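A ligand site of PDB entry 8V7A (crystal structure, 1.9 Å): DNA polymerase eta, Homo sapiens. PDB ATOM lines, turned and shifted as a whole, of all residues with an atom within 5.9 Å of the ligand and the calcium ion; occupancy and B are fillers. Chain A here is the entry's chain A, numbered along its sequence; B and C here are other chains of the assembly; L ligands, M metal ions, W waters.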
ATOM      1  N   ASP A  16       6.943   3.875 -35.827  1.00  0.00           N
ATOM      2  CA  ASP A  16       7.138   3.731 -34.387  1.00  0.00           C
ATOM      3  C   ASP A  16       8.468   4.342 -33.981  1.00  0.00           C
ATOM      4  O   ASP A  16       9.510   3.992 -34.533  1.00  0.00           O
ATOM      5  CB  ASP A  16       7.132   2.266 -33.973  1.00  0.00           C
ATOM      6  CG  ASP A  16       7.669   2.073 -32.565  1.00  0.00           C
ATOM      7  OD1 ASP A  16       8.886   1.949 -32.357  1.00  0.00           O
ATOM      8  OD2 ASP A  16       6.839   2.052 -31.651  1.00  0.00           O
ATOM      9  N   MET A  17       8.463   5.199 -32.969  1.00  0.00           N
ATOM     10  CA  MET A  17       9.697   5.880 -32.592  1.00  0.00           C
ATOM     11  C   MET A  17      10.588   4.893 -31.853  1.00  0.00           C
ATOM     12  O   MET A  17      10.115   4.088 -31.042  1.00  0.00           O
ATOM     13  CB  MET A  17       9.407   7.098 -31.704  1.00  0.00           C
ATOM     14  CG  MET A  17       8.368   8.063 -32.311  1.00  0.00           C
ATOM     15  SD  MET A  17       8.857   8.678 -33.925  1.00  0.00           S
ATOM     16  CE  MET A  17      10.512   9.193 -33.612  1.00  0.00           C
ATOM     17  N   ASP A  18      11.894   4.936 -32.140  1.00  0.00           N
ATOM     18  CA  ASP A  18      12.853   4.071 -31.417  1.00  0.00           C
ATOM     19  C   ASP A  18      13.014   4.577 -29.975  1.00  0.00           C
ATOM     20  O   ASP A  18      13.098   5.798 -29.871  1.00  0.00           O
ATOM     21  CB  ASP A  18      14.171   4.015 -32.179  1.00  0.00           C
ATOM     22  CG  ASP A  18      14.039   3.468 -33.584  1.00  0.00           C
ATOM     23  OD1 ASP A  18      13.157   2.632 -33.809  1.00  0.00           O
ATOM     24  OD2 ASP A  18      14.825   3.881 -34.447  1.00  0.00           O
ATOM     25  N   CYS A  19      13.033   3.679 -28.963  1.00  0.00           N
ATOM     26  CA  CYS A  19      13.208   4.008 -27.508  1.00  0.00           C
ATOM     27  C   CYS A  19      12.706   5.423 -27.225  1.00  0.00           C
ATOM     28  O   CYS A  19      13.481   6.246 -26.786  1.00  0.00           O
ATOM     29  CB  CYS A  19      14.670   3.829 -27.096  1.00  0.00           C
ATOM     30  SG  CYS A  19      15.891   4.624 -28.166  1.00  0.00           S
ATOM     31  N   PHE A  20      11.432   5.653 -27.528  1.00  0.00           N
ATOM     32  CA  PHE A  20      10.905   7.036 -27.548  1.00  0.00           C
ATOM     33  C   PHE A  20      11.301   7.884 -26.348  1.00  0.00           C
ATOM     34  O   PHE A  20      11.910   8.925 -26.565  1.00  0.00           O
ATOM     35  CB  PHE A  20       9.401   7.066 -27.755  1.00  0.00           C
ATOM     36  CG  PHE A  20       8.855   8.445 -28.011  1.00  0.00           C
ATOM     37  CD1 PHE A  20       9.482   9.284 -28.913  1.00  0.00           C
ATOM     38  CD2 PHE A  20       7.744   8.910 -27.336  1.00  0.00           C
ATOM     39  CE1 PHE A  20       8.989  10.560 -29.148  1.00  0.00           C
ATOM     40  CE2 PHE A  20       7.252  10.186 -27.571  1.00  0.00           C
ATOM     41  CZ  PHE A  20       7.880  11.011 -28.473  1.00  0.00           C
ATOM     42  N   PHE A  21      10.911   7.503 -25.119  1.00  0.00           N
ATOM     43  CA  PHE A  21      11.162   8.447 -24.033  1.00  0.00           C
ATOM     44  C   PHE A  21      12.664   8.695 -23.845  1.00  0.00           C
ATOM     45  O   PHE A  21      13.082   9.811 -23.487  1.00  0.00           O
ATOM     46  CB  PHE A  21      10.561   7.961 -22.710  1.00  0.00           C
ATOM     47  CG  PHE A  21       9.058   8.029 -22.641  1.00  0.00           C
ATOM     48  CD1 PHE A  21       8.290   8.186 -23.783  1.00  0.00           C
ATOM     49  CD2 PHE A  21       8.427   7.886 -21.417  1.00  0.00           C
ATOM     50  CE1 PHE A  21       6.882   8.241 -23.692  1.00  0.00           C
ATOM     51  CE2 PHE A  21       7.046   7.908 -21.324  1.00  0.00           C
ATOM     52  CZ  PHE A  21       6.286   8.108 -22.457  1.00  0.00           C
ATOM     53  N   VAL A  22      13.476   7.683 -24.138  1.00  0.00           N
ATOM     54  CA  VAL A  22      14.934   7.840 -24.094  1.00  0.00           C
ATOM     55  C   VAL A  22      15.385   8.901 -25.103  1.00  0.00           C
ATOM     56  O   VAL A  22      16.206   9.770 -24.783  1.00  0.00           O
ATOM     57  CB  VAL A  22      15.628   6.493 -24.332  1.00  0.00           C
ATOM     58  CG1 VAL A  22      17.093   6.724 -24.629  1.00  0.00           C
ATOM     59  CG2 VAL A  22      15.515   5.599 -23.083  1.00  0.00           C
ATOM     60  N   ILE A  51      11.132   2.666 -17.496  1.00  0.00           N
ATOM     61  CA  ILE A  51      10.045   2.626 -18.480  1.00  0.00           C
ATOM     62  C   ILE A  51      10.521   2.692 -19.926  1.00  0.00           C
ATOM     63  O   ILE A  51       9.734   2.388 -20.836  1.00  0.00           O
ATOM     64  CB  ILE A  51       8.985   3.713 -18.201  1.00  0.00           C
ATOM     65  CG1 ILE A  51       9.567   5.123 -18.300  1.00  0.00           C
ATOM     66  CG2 ILE A  51       8.355   3.491 -16.808  1.00  0.00           C
ATOM     67  CD1 ILE A  51       8.476   6.193 -18.196  1.00  0.00           C
ATOM     68  N   ALA A  52      11.783   3.035 -20.194  1.00  0.00           N
ATOM     69  CA  ALA A  52      12.306   3.024 -21.561  1.00  0.00           C
ATOM     70  C   ALA A  52      13.808   2.822 -21.504  1.00  0.00           C
ATOM     71  O   ALA A  52      14.454   3.266 -20.548  1.00  0.00           O
ATOM     72  CB  ALA A  52      11.985   4.340 -22.288  1.00  0.00           C
ATOM     73  N   VAL A  53      14.366   2.173 -22.530  1.00  0.00           N
ATOM     74  CA  VAL A  53      15.741   1.668 -22.514  1.00  0.00           C
ATOM     75  C   VAL A  53      16.396   1.905 -23.867  1.00  0.00           C
ATOM     76  O   VAL A  53      15.858   1.483 -24.907  1.00  0.00           O
ATOM     77  CB  VAL A  53      15.770   0.162 -22.190  1.00  0.00           C
ATOM     78  CG1 VAL A  53      17.209  -0.302 -21.989  1.00  0.00           C
ATOM     79  CG2 VAL A  53      14.922  -0.145 -21.001  1.00  0.00           C
ATOM     80  N   TYR A  55      19.102   1.346 -26.943  1.00  0.00           N
ATOM     81  CA  TYR A  55      19.560   0.082 -27.519  1.00  0.00           C
ATOM     82  C   TYR A  55      20.934  -0.311 -26.996  1.00  0.00           C
ATOM     83  O   TYR A  55      21.219  -1.514 -26.799  1.00  0.00           O
ATOM     84  CB  TYR A  55      19.542   0.143 -29.059  1.00  0.00           C
ATOM     85  CG  TYR A  55      18.125   0.049 -29.615  1.00  0.00           C
ATOM     86  CD1 TYR A  55      17.189   1.066 -29.420  1.00  0.00           C
ATOM     87  CD2 TYR A  55      17.660  -1.151 -30.129  1.00  0.00           C
ATOM     88  CE1 TYR A  55      15.858   0.934 -29.869  1.00  0.00           C
ATOM     89  CE2 TYR A  55      16.345  -1.318 -30.559  1.00  0.00           C
ATOM     90  CZ  TYR A  55      15.448  -0.271 -30.444  1.00  0.00           C
ATOM     91  OH  TYR A  55      14.142  -0.473 -30.896  1.00  0.00           O
ATOM     92  N   ARG A  58      20.052  -2.021 -23.821  1.00  0.00           N
ATOM     93  CA  ARG A  58      19.471  -3.352 -24.067  1.00  0.00           C
ATOM     94  C   ARG A  58      20.546  -4.403 -24.309  1.00  0.00           C
ATOM     95  O   ARG A  58      20.344  -5.572 -23.937  1.00  0.00           O
ATOM     96  CB  ARG A  58      18.517  -3.326 -25.244  1.00  0.00           C
ATOM     97  CG  ARG A  58      17.354  -2.397 -25.035  1.00  0.00           C
ATOM     98  CD  ARG A  58      16.533  -2.290 -26.287  1.00  0.00           C
ATOM     99  NE  ARG A  58      15.659  -1.134 -26.180  1.00  0.00           N
ATOM    100  CZ  ARG A  58      14.626  -0.907 -26.960  1.00  0.00           C
ATOM    101  NH1 ARG A  58      14.242  -1.781 -27.884  1.00  0.00           N
ATOM    102  NH2 ARG A  58      13.949   0.232 -26.805  1.00  0.00           N
ATOM    103  N   ARG A  64      12.557  -2.937 -19.653  1.00  0.00           N
ATOM    104  CA  ARG A  64      11.467  -2.271 -18.955  1.00  0.00           C
ATOM    105  C   ARG A  64      10.986  -3.136 -17.776  1.00  0.00           C
ATOM    106  O   ARG A  64      11.153  -4.358 -17.761  1.00  0.00           O
ATOM    107  CB  ARG A  64      10.335  -2.002 -19.956  1.00  0.00           C
ATOM    108  CG  ARG A  64       9.023  -1.523 -19.416  1.00  0.00           C
ATOM    109  CD  ARG A  64       8.078  -1.241 -20.583  1.00  0.00           C
ATOM    110  NE  ARG A  64       8.614  -0.159 -21.396  1.00  0.00           N
ATOM    111  CZ  ARG A  64       8.781  -0.188 -22.713  1.00  0.00           C
ATOM    112  NH1 ARG A  64       8.482  -1.247 -23.428  1.00  0.00           N
ATOM    113  NH2 ARG A  64       9.266   0.887 -23.322  1.00  0.00           N
ATOM    114  N   SER A 116      -0.693   5.252 -30.430  1.00  0.00           N
ATOM    115  CA  SER A 116      -0.078   5.376 -29.092  1.00  0.00           C
ATOM    116  C   SER A 116       0.712   6.679 -29.015  1.00  0.00           C
ATOM    117  O   SER A 116       0.783   7.387 -30.015  1.00  0.00           O
ATOM    118  CB  SER A 116       0.841   4.208 -28.841  1.00  0.00           C
ATOM    119  OG  SER A 116       2.098   4.417 -29.445  1.00  0.00           O
ATOM    120  N   ILE A 117       1.308   6.931 -27.862  1.00  0.00           N
ATOM    121  CA  ILE A 117       2.135   8.149 -27.701  1.00  0.00           C
ATOM    122  C   ILE A 117       3.204   8.182 -28.796  1.00  0.00           C
ATOM    123  O   ILE A 117       3.630   9.282 -29.155  1.00  0.00           O
ATOM    124  CB  ILE A 117       2.805   8.219 -26.310  1.00  0.00           C
ATOM    125  CG1 ILE A 117       3.363   9.617 -26.036  1.00  0.00           C
ATOM    126  CG2 ILE A 117       3.877   7.149 -26.143  1.00  0.00           C
ATOM    127  CD1 ILE A 117       3.289  10.035 -24.594  1.00  0.00           C
ATOM    128  N   ASP A 118       3.678   7.046 -29.336  1.00  0.00           N
ATOM    129  CA  ASP A 118       4.821   7.086 -30.243  1.00  0.00           C
ATOM    130  C   ASP A 118       4.625   6.241 -31.508  1.00  0.00           C
ATOM    131  O   ASP A 118       5.623   5.906 -32.180  1.00  0.00           O
ATOM    132  CB  ASP A 118       6.111   6.648 -29.552  1.00  0.00           C
ATOM    133  CG  ASP A 118       6.237   5.134 -29.464  1.00  0.00           C
ATOM    134  OD1 ASP A 118       5.188   4.470 -29.324  1.00  0.00           O
ATOM    135  OD2 ASP A 118       7.371   4.602 -29.553  1.00  0.00           O
ATOM    136  N   GLU A 119       3.395   5.878 -31.837  1.00  0.00           N
ATOM    137  CA  GLU A 119       3.068   5.087 -33.035  1.00  0.00           C
ATOM    138  C   GLU A 119       1.870   5.692 -33.757  1.00  0.00           C
ATOM    139  O   GLU A 119       0.914   6.111 -33.097  1.00  0.00           O
ATOM    140  CB  GLU A 119       2.604   3.672 -32.710  1.00  0.00           C
ATOM    141  CG  GLU A 119       3.565   2.832 -31.913  1.00  0.00           C
ATOM    142  CD  GLU A 119       3.091   1.412 -31.666  1.00  0.00           C
ATOM    143  OE1 GLU A 119       1.998   1.056 -32.133  1.00  0.00           O
ATOM    144  OE2 GLU A 119       3.834   0.691 -31.003  1.00  0.00           O
ATOM    145  N   LYS A 234      14.824  -3.171 -36.180  1.00  0.00           N
ATOM    146  CA  LYS A 234      14.899  -1.933 -35.383  1.00  0.00           C
ATOM    147  C   LYS A 234      16.353  -1.952 -34.911  1.00  0.00           C
ATOM    148  O   LYS A 234      17.052  -3.001 -34.819  1.00  0.00           O
ATOM    149  CB  LYS A 234      13.893  -1.977 -34.227  1.00  0.00           C
ATOM    150  CG  LYS A 234      12.470  -1.569 -34.566  1.00  0.00           C
ATOM    151  CD  LYS A 234      11.801  -0.895 -33.394  1.00  0.00           C
ATOM    152  CE  LYS A 234      10.371  -1.338 -33.194  1.00  0.00           C
ATOM    153  NZ  LYS A 234       9.426  -0.404 -33.841  1.00  0.00           N
ATOM    154  N   PRO A 235      16.888  -0.799 -34.477  1.00  0.00           N
ATOM    155  CA  PRO A 235      16.282   0.527 -34.658  1.00  0.00           C
ATOM    156  C   PRO A 235      16.623   1.193 -36.004  1.00  0.00           C
ATOM    157  O   PRO A 235      17.482   0.705 -36.754  1.00  0.00           O
ATOM    158  CB  PRO A 235      16.886   1.313 -33.489  1.00  0.00           C
ATOM    159  CG  PRO A 235      18.297   0.737 -33.389  1.00  0.00           C
ATOM    160  CD  PRO A 235      18.166  -0.727 -33.749  1.00  0.00           C
ATOM    161  P    DT B   3       6.406  -5.655  -8.298  1.00  0.00           P
ATOM    162  OP1  DT B   3       5.864  -6.814  -7.533  1.00  0.00           O
ATOM    163  OP2  DT B   3       7.782  -5.707  -8.846  1.00  0.00           O
ATOM    164  O5'  DT B   3       5.377  -5.366  -9.493  1.00  0.00           O
ATOM    165  C5'  DT B   3       5.805  -4.643 -10.636  1.00  0.00           C
ATOM    166  C4'  DT B   3       5.957  -3.176 -10.310  1.00  0.00           C
ATOM    167  O4'  DT B   3       6.854  -2.541 -11.256  1.00  0.00           O
ATOM    168  C3'  DT B   3       4.653  -2.364 -10.342  1.00  0.00           C
ATOM    169  O3'  DT B   3       4.620  -1.478  -9.249  1.00  0.00           O
ATOM    170  C2'  DT B   3       4.777  -1.594 -11.646  1.00  0.00           C
ATOM    171  C1'  DT B   3       6.264  -1.324 -11.676  1.00  0.00           C
ATOM    172  N1   DT B   3       6.758  -1.004 -13.024  1.00  0.00           N
ATOM    173  C2   DT B   3       7.630   0.049 -13.207  1.00  0.00           C
ATOM    174  O2   DT B   3       8.043   0.748 -12.296  1.00  0.00           O
ATOM    175  N3   DT B   3       8.000   0.247 -14.516  1.00  0.00           N
ATOM    176  C4   DT B   3       7.597  -0.485 -15.625  1.00  0.00           C
ATOM    177  O4   DT B   3       7.971  -0.231 -16.747  1.00  0.00           O
ATOM    178  C5   DT B   3       6.681  -1.568 -15.354  1.00  0.00           C
ATOM    179  C7   DT B   3       6.173  -2.417 -16.482  1.00  0.00           C
ATOM    180  C6   DT B   3       6.315  -1.771 -14.091  1.00  0.00           C
ATOM    181  P    DG B   4       3.378  -0.477  -9.069  1.00  0.00           P
ATOM    182  OP1  DG B   4       3.437   0.122  -7.715  1.00  0.00           O
ATOM    183  OP2  DG B   4       2.189  -1.205  -9.566  1.00  0.00           O
ATOM    184  O5'  DG B   4       3.650   0.654 -10.147  1.00  0.00           O
ATOM    185  C5'  DG B   4       4.669   1.606  -9.966  1.00  0.00           C
ATOM    186  C4'  DG B   4       4.379   2.825 -10.826  1.00  0.00           C
ATOM    187  O4'  DG B   4       4.602   2.506 -12.223  1.00  0.00           O
ATOM    188  C3'  DG B   4       2.940   3.326 -10.752  1.00  0.00           C
ATOM    189  O3'  DG B   4       2.955   4.704 -10.969  1.00  0.00           O
ATOM    190  C2'  DG B   4       2.273   2.583 -11.919  1.00  0.00           C
ATOM    191  C1'  DG B   4       3.386   2.662 -12.958  1.00  0.00           C
ATOM    192  N9   DG B   4       3.375   1.626 -13.988  1.00  0.00           N
ATOM    193  C8   DG B   4       3.048   0.297 -13.853  1.00  0.00           C
ATOM    194  N7   DG B   4       3.198  -0.384 -14.957  1.00  0.00           N
ATOM    195  C5   DG B   4       3.679   0.561 -15.866  1.00  0.00           C
ATOM    196  C6   DG B   4       4.054   0.414 -17.233  1.00  0.00           C
ATOM    197  O6   DG B   4       4.013  -0.605 -17.938  1.00  0.00           O
ATOM    198  N1   DG B   4       4.481   1.636 -17.768  1.00  0.00           N
ATOM    199  C2   DG B   4       4.568   2.816 -17.076  1.00  0.00           C
ATOM    200  N2   DG B   4       5.015   3.882 -17.745  1.00  0.00           N
ATOM    201  N3   DG B   4       4.236   2.944 -15.802  1.00  0.00           N
ATOM    202  C4   DG B   4       3.804   1.778 -15.265  1.00  0.00           C
ATOM    203  P    DA B   5       1.627   5.596 -10.947  1.00  0.00           P
ATOM    204  OP1  DA B   5       2.005   6.767 -10.171  1.00  0.00           O
ATOM    205  OP2  DA B   5       0.431   4.793 -10.583  1.00  0.00           O
ATOM    206  O5'  DA B   5       1.441   6.031 -12.491  1.00  0.00           O
ATOM    207  C5'  DA B   5       2.434   6.867 -13.095  1.00  0.00           C
ATOM    208  C4'  DA B   5       2.072   7.214 -14.521  1.00  0.00           C
ATOM    209  O4'  DA B   5       2.233   6.031 -15.355  1.00  0.00           O
ATOM    210  C3'  DA B   5       0.623   7.676 -14.706  1.00  0.00           C
ATOM    211  O3'  DA B   5       0.564   8.683 -15.694  1.00  0.00           O
ATOM    212  C2'  DA B   5      -0.058   6.402 -15.173  1.00  0.00           C
ATOM    213  C1'  DA B   5       1.038   5.802 -16.049  1.00  0.00           C
ATOM    214  N9   DA B   5       0.886   4.375 -16.300  1.00  0.00           N
ATOM    215  C8   DA B   5       0.485   3.424 -15.412  1.00  0.00           C
ATOM    216  N7   DA B   5       0.447   2.212 -15.912  1.00  0.00           N
ATOM    217  C5   DA B   5       0.849   2.378 -17.227  1.00  0.00           C
ATOM    218  C6   DA B   5       1.009   1.474 -18.279  1.00  0.00           C
ATOM    219  N6   DA B   5       0.766   0.169 -18.148  1.00  0.00           N
ATOM    220  N1   DA B   5       1.426   1.949 -19.469  1.00  0.00           N
ATOM    221  C2   DA B   5       1.668   3.261 -19.588  1.00  0.00           C
ATOM    222  N3   DA B   5       1.549   4.217 -18.659  1.00  0.00           N
ATOM    223  C4   DA B   5       1.129   3.700 -17.487  1.00  0.00           C
ATOM    224  P    DT C   8       2.475  -2.946 -27.874  1.00  0.00           P
ATOM    225  OP1  DT C   8       3.306  -3.008 -29.126  1.00  0.00           O
ATOM    226  OP2  DT C   8       3.032  -3.737 -26.719  1.00  0.00           O
ATOM    227  O5'  DT C   8       2.437  -1.413 -27.398  1.00  0.00           O
ATOM    228  C5'  DT C   8       1.857  -0.416 -28.261  1.00  0.00           C
ATOM    229  C4'  DT C   8       2.073   0.937 -27.636  1.00  0.00           C
ATOM    230  O4'  DT C   8       1.451   0.969 -26.328  1.00  0.00           O
ATOM    231  C3'  DT C   8       3.538   1.323 -27.432  1.00  0.00           C
ATOM    232  O3'  DT C   8       3.732   2.677 -27.812  1.00  0.00           O
ATOM    233  C2'  DT C   8       3.765   1.129 -25.943  1.00  0.00           C
ATOM    234  C1'  DT C   8       2.390   1.400 -25.357  1.00  0.00           C
ATOM    235  N1   DT C   8       2.104   0.659 -24.116  1.00  0.00           N
ATOM    236  C2   DT C   8       1.906   1.382 -22.955  1.00  0.00           C
ATOM    237  O2   DT C   8       1.952   2.603 -22.922  1.00  0.00           O
ATOM    238  N3   DT C   8       1.647   0.629 -21.851  1.00  0.00           N
ATOM    239  C4   DT C   8       1.567  -0.749 -21.769  1.00  0.00           C
ATOM    240  O4   DT C   8       1.325  -1.286 -20.691  1.00  0.00           O
ATOM    241  C5   DT C   8       1.792  -1.445 -23.018  1.00  0.00           C
ATOM    242  C7   DT C   8       1.719  -2.940 -23.027  1.00  0.00           C
ATOM    243  C6   DT C   8       2.041  -0.714 -24.117  1.00  0.00           C
HETATM  244  N1  LIG L   1       5.925   2.966 -22.420  1.00  0.00           N
HETATM  245  C1  LIG L   1       5.585   2.883 -21.068  1.00  0.00           C
HETATM  246  N2  LIG L   1       5.201   1.695 -20.551  1.00  0.00           N
HETATM  247  C2  LIG L   1       5.145   0.608 -21.331  1.00  0.00           C
HETATM  248  C3  LIG L   1       5.496   0.672 -22.713  1.00  0.00           C
HETATM  249  C4  LIG L   1       5.882   1.859 -23.206  1.00  0.00           C
HETATM  250  O1  LIG L   1       5.654   3.906 -20.382  1.00  0.00           O
HETATM  251  N3  LIG L   1       4.758  -0.533 -20.776  1.00  0.00           N
HETATM  252  C5  LIG L   1       6.360   4.268 -22.964  1.00  0.00           C
HETATM  253  C6  LIG L   1       7.861   4.507 -22.907  1.00  0.00           C
HETATM  254  C7  LIG L   1       8.314   4.105 -24.301  1.00  0.00           C
HETATM  255  C8  LIG L   1       7.138   4.527 -25.159  1.00  0.00           C
HETATM  256  O2  LIG L   1       5.972   4.353 -24.317  1.00  0.00           O
HETATM  257  O3  LIG L   1       9.486   4.800 -24.680  1.00  0.00           O
HETATM  258  C9  LIG L   1       6.965   3.734 -26.428  1.00  0.00           C
HETATM  259  O4  LIG L   1       6.832   2.338 -26.073  1.00  0.00           O
HETATM  260  P1  LIG L   1       7.346   1.205 -27.061  1.00  0.00           P
HETATM  261  O5  LIG L   1       7.227   1.677 -28.464  1.00  0.00           O
HETATM  262  O6  LIG L   1       6.701  -0.082 -26.692  1.00  0.00           O
HETATM  263  O7  LIG L   1       8.902   1.145 -26.696  1.00  0.00           O
HETATM  264  P2  LIG L   1      10.130   2.126 -26.986  1.00  0.00           P
HETATM  265  O8  LIG L   1       9.716   3.138 -27.969  1.00  0.00           O
HETATM  266  O9  LIG L   1      10.687   2.552 -25.685  1.00  0.00           O
HETATM  267  O10 LIG L   1      11.171   1.119 -27.657  1.00  0.00           O
HETATM  268  P3  LIG L   1      11.206   0.456 -29.114  1.00  0.00           P
HETATM  269  O11 LIG L   1       9.892   0.782 -29.738  1.00  0.00           O
HETATM  270  O12 LIG L   1      12.362   1.072 -29.819  1.00  0.00           O
HETATM  271  O13 LIG L   1      11.392  -1.007 -28.900  1.00  0.00           O
HETATM  272 CA    CA M   1       8.589   2.714 -29.988  1.00  0.00          CA
HETATM  273  O   HOH W   1       5.290  -2.976 -22.475  1.00  0.00           O
HETATM  274  O   HOH W   2      10.602  -2.363 -26.715  1.00  0.00           O
HETATM  275  O   HOH W   3       3.023   5.041 -23.526  1.00  0.00           O
HETATM  276  O   HOH W   4       5.095  -1.964 -25.142  1.00  0.00           O
HETATM  277  O   HOH W   5       8.248  -2.271 -26.012  1.00  0.00           O
HETATM  278  O   HOH W   6      12.288   1.173 -24.256  1.00  0.00           O
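CA of Asp 18 touches O12 of the ligand, at 3.4 Å.
Ile 51 touches the ligand (O to C6, 3.5 Å).
Ala 52 touches the ligand.
Ile 117 touches the ligand (CG2 to O2, 3.9 Å).
DA 5 of chain B touches the ligand.
16 residues have an atom within 4 Å of the ligand: Asp 16, Met 17, Asp 18, Cys 19, Phe 20, Phe 21, Ile 51, Ala 52, Tyr 55, Arg 58, Arg 64, Ile 117, Asp 118, DG 4 of chain B, DA 5 of chain B and DT 8 of chain C.
The nearest printed residue that does not touch the ligand is Lys 234 (4.1 Å).
Of the 23 residues printed, 3 come within 4 Å of the calcium ion.
The calcium ion is bound by OD2 of Asp 118 (2.3 Å), O5 of the ligand (2.3 Å), O of Met 17 (2.3 Å), O11 of the ligand (2.3 Å), O8 of the ligand (2.4 Å), OD2 of Asp 16 (2.5 Å) and OD1 of Asp 16 (2.5 Å).
The calcium ion has seven donor atoms within binding distance.
Water W5 lies within hydrogen-bond range of O6 of the ligand (2.8 Å) and NH1 of Arg 64 (2.8 Å).
Water W4 lies within hydrogen-bond range of O6 of the ligand and OP2 of DT 8 of chain C.
Water W3 bridges O2 of DT 8 of chain C and O2 of the ligand.
N of Asp 118 sits close to OG of Ser 116 (3.1 Å).
The side-chain carboxylate (OD1) of Asp 16 lies close to the side-chain amino group (NZ) of Lys 234, 2.8 Å away.
The side-chain hydroxyl of Tyr 55 sits close to the guanidinium group of Arg 58.
The guanidinium group of Arg 58 lies within hydrogen-bond range of the backbone carbonyl oxygen of Val 53 (2.9 Å).
The guanidinium group (NE) of Arg 64 lies within hydrogen-bond range of the backbone carbonyl oxygen (O) of Ile 51 (2.8 Å).
N3 of DT 8 of chain C sits close to N1 of DA 5 of chain B (2.7 Å).
O3' of DT 8 of chain C lies within hydrogen-bond range of OG of Ser 116, 2.9 Å away.
The side-chain hydroxyl of Tyr 55 sits at hydrogen-bond distance from an oxygen (O12) of the ligand, 2.6 Å away.
N3 of the ligand sits at hydrogen-bond distance from O6 of DG 4 of chain B (2.9 Å).
The backbone NH of Cys 19 lies within hydrogen-bond range of an oxygen (O12) of the ligand (2.8 Å).
O13 of the ligand is in salt-bridge range of NH1 of Arg 58 (3.1 Å).
An oxygen (O8) of the ligand lies close to the backbone NH (N) of Phe 20.
The backbone NH of Phe 21 sits at hydrogen-bond distance from an oxygen (O3) of the ligand (3.1 Å).
An oxygen (O9) of the ligand lies within salt-bridge range of the guanidinium group (NH2) of Arg 64 (3.2 Å).
A nitrogen (N3) of the ligand sits close to N3 of DT 8 of chain C (3.5 Å).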
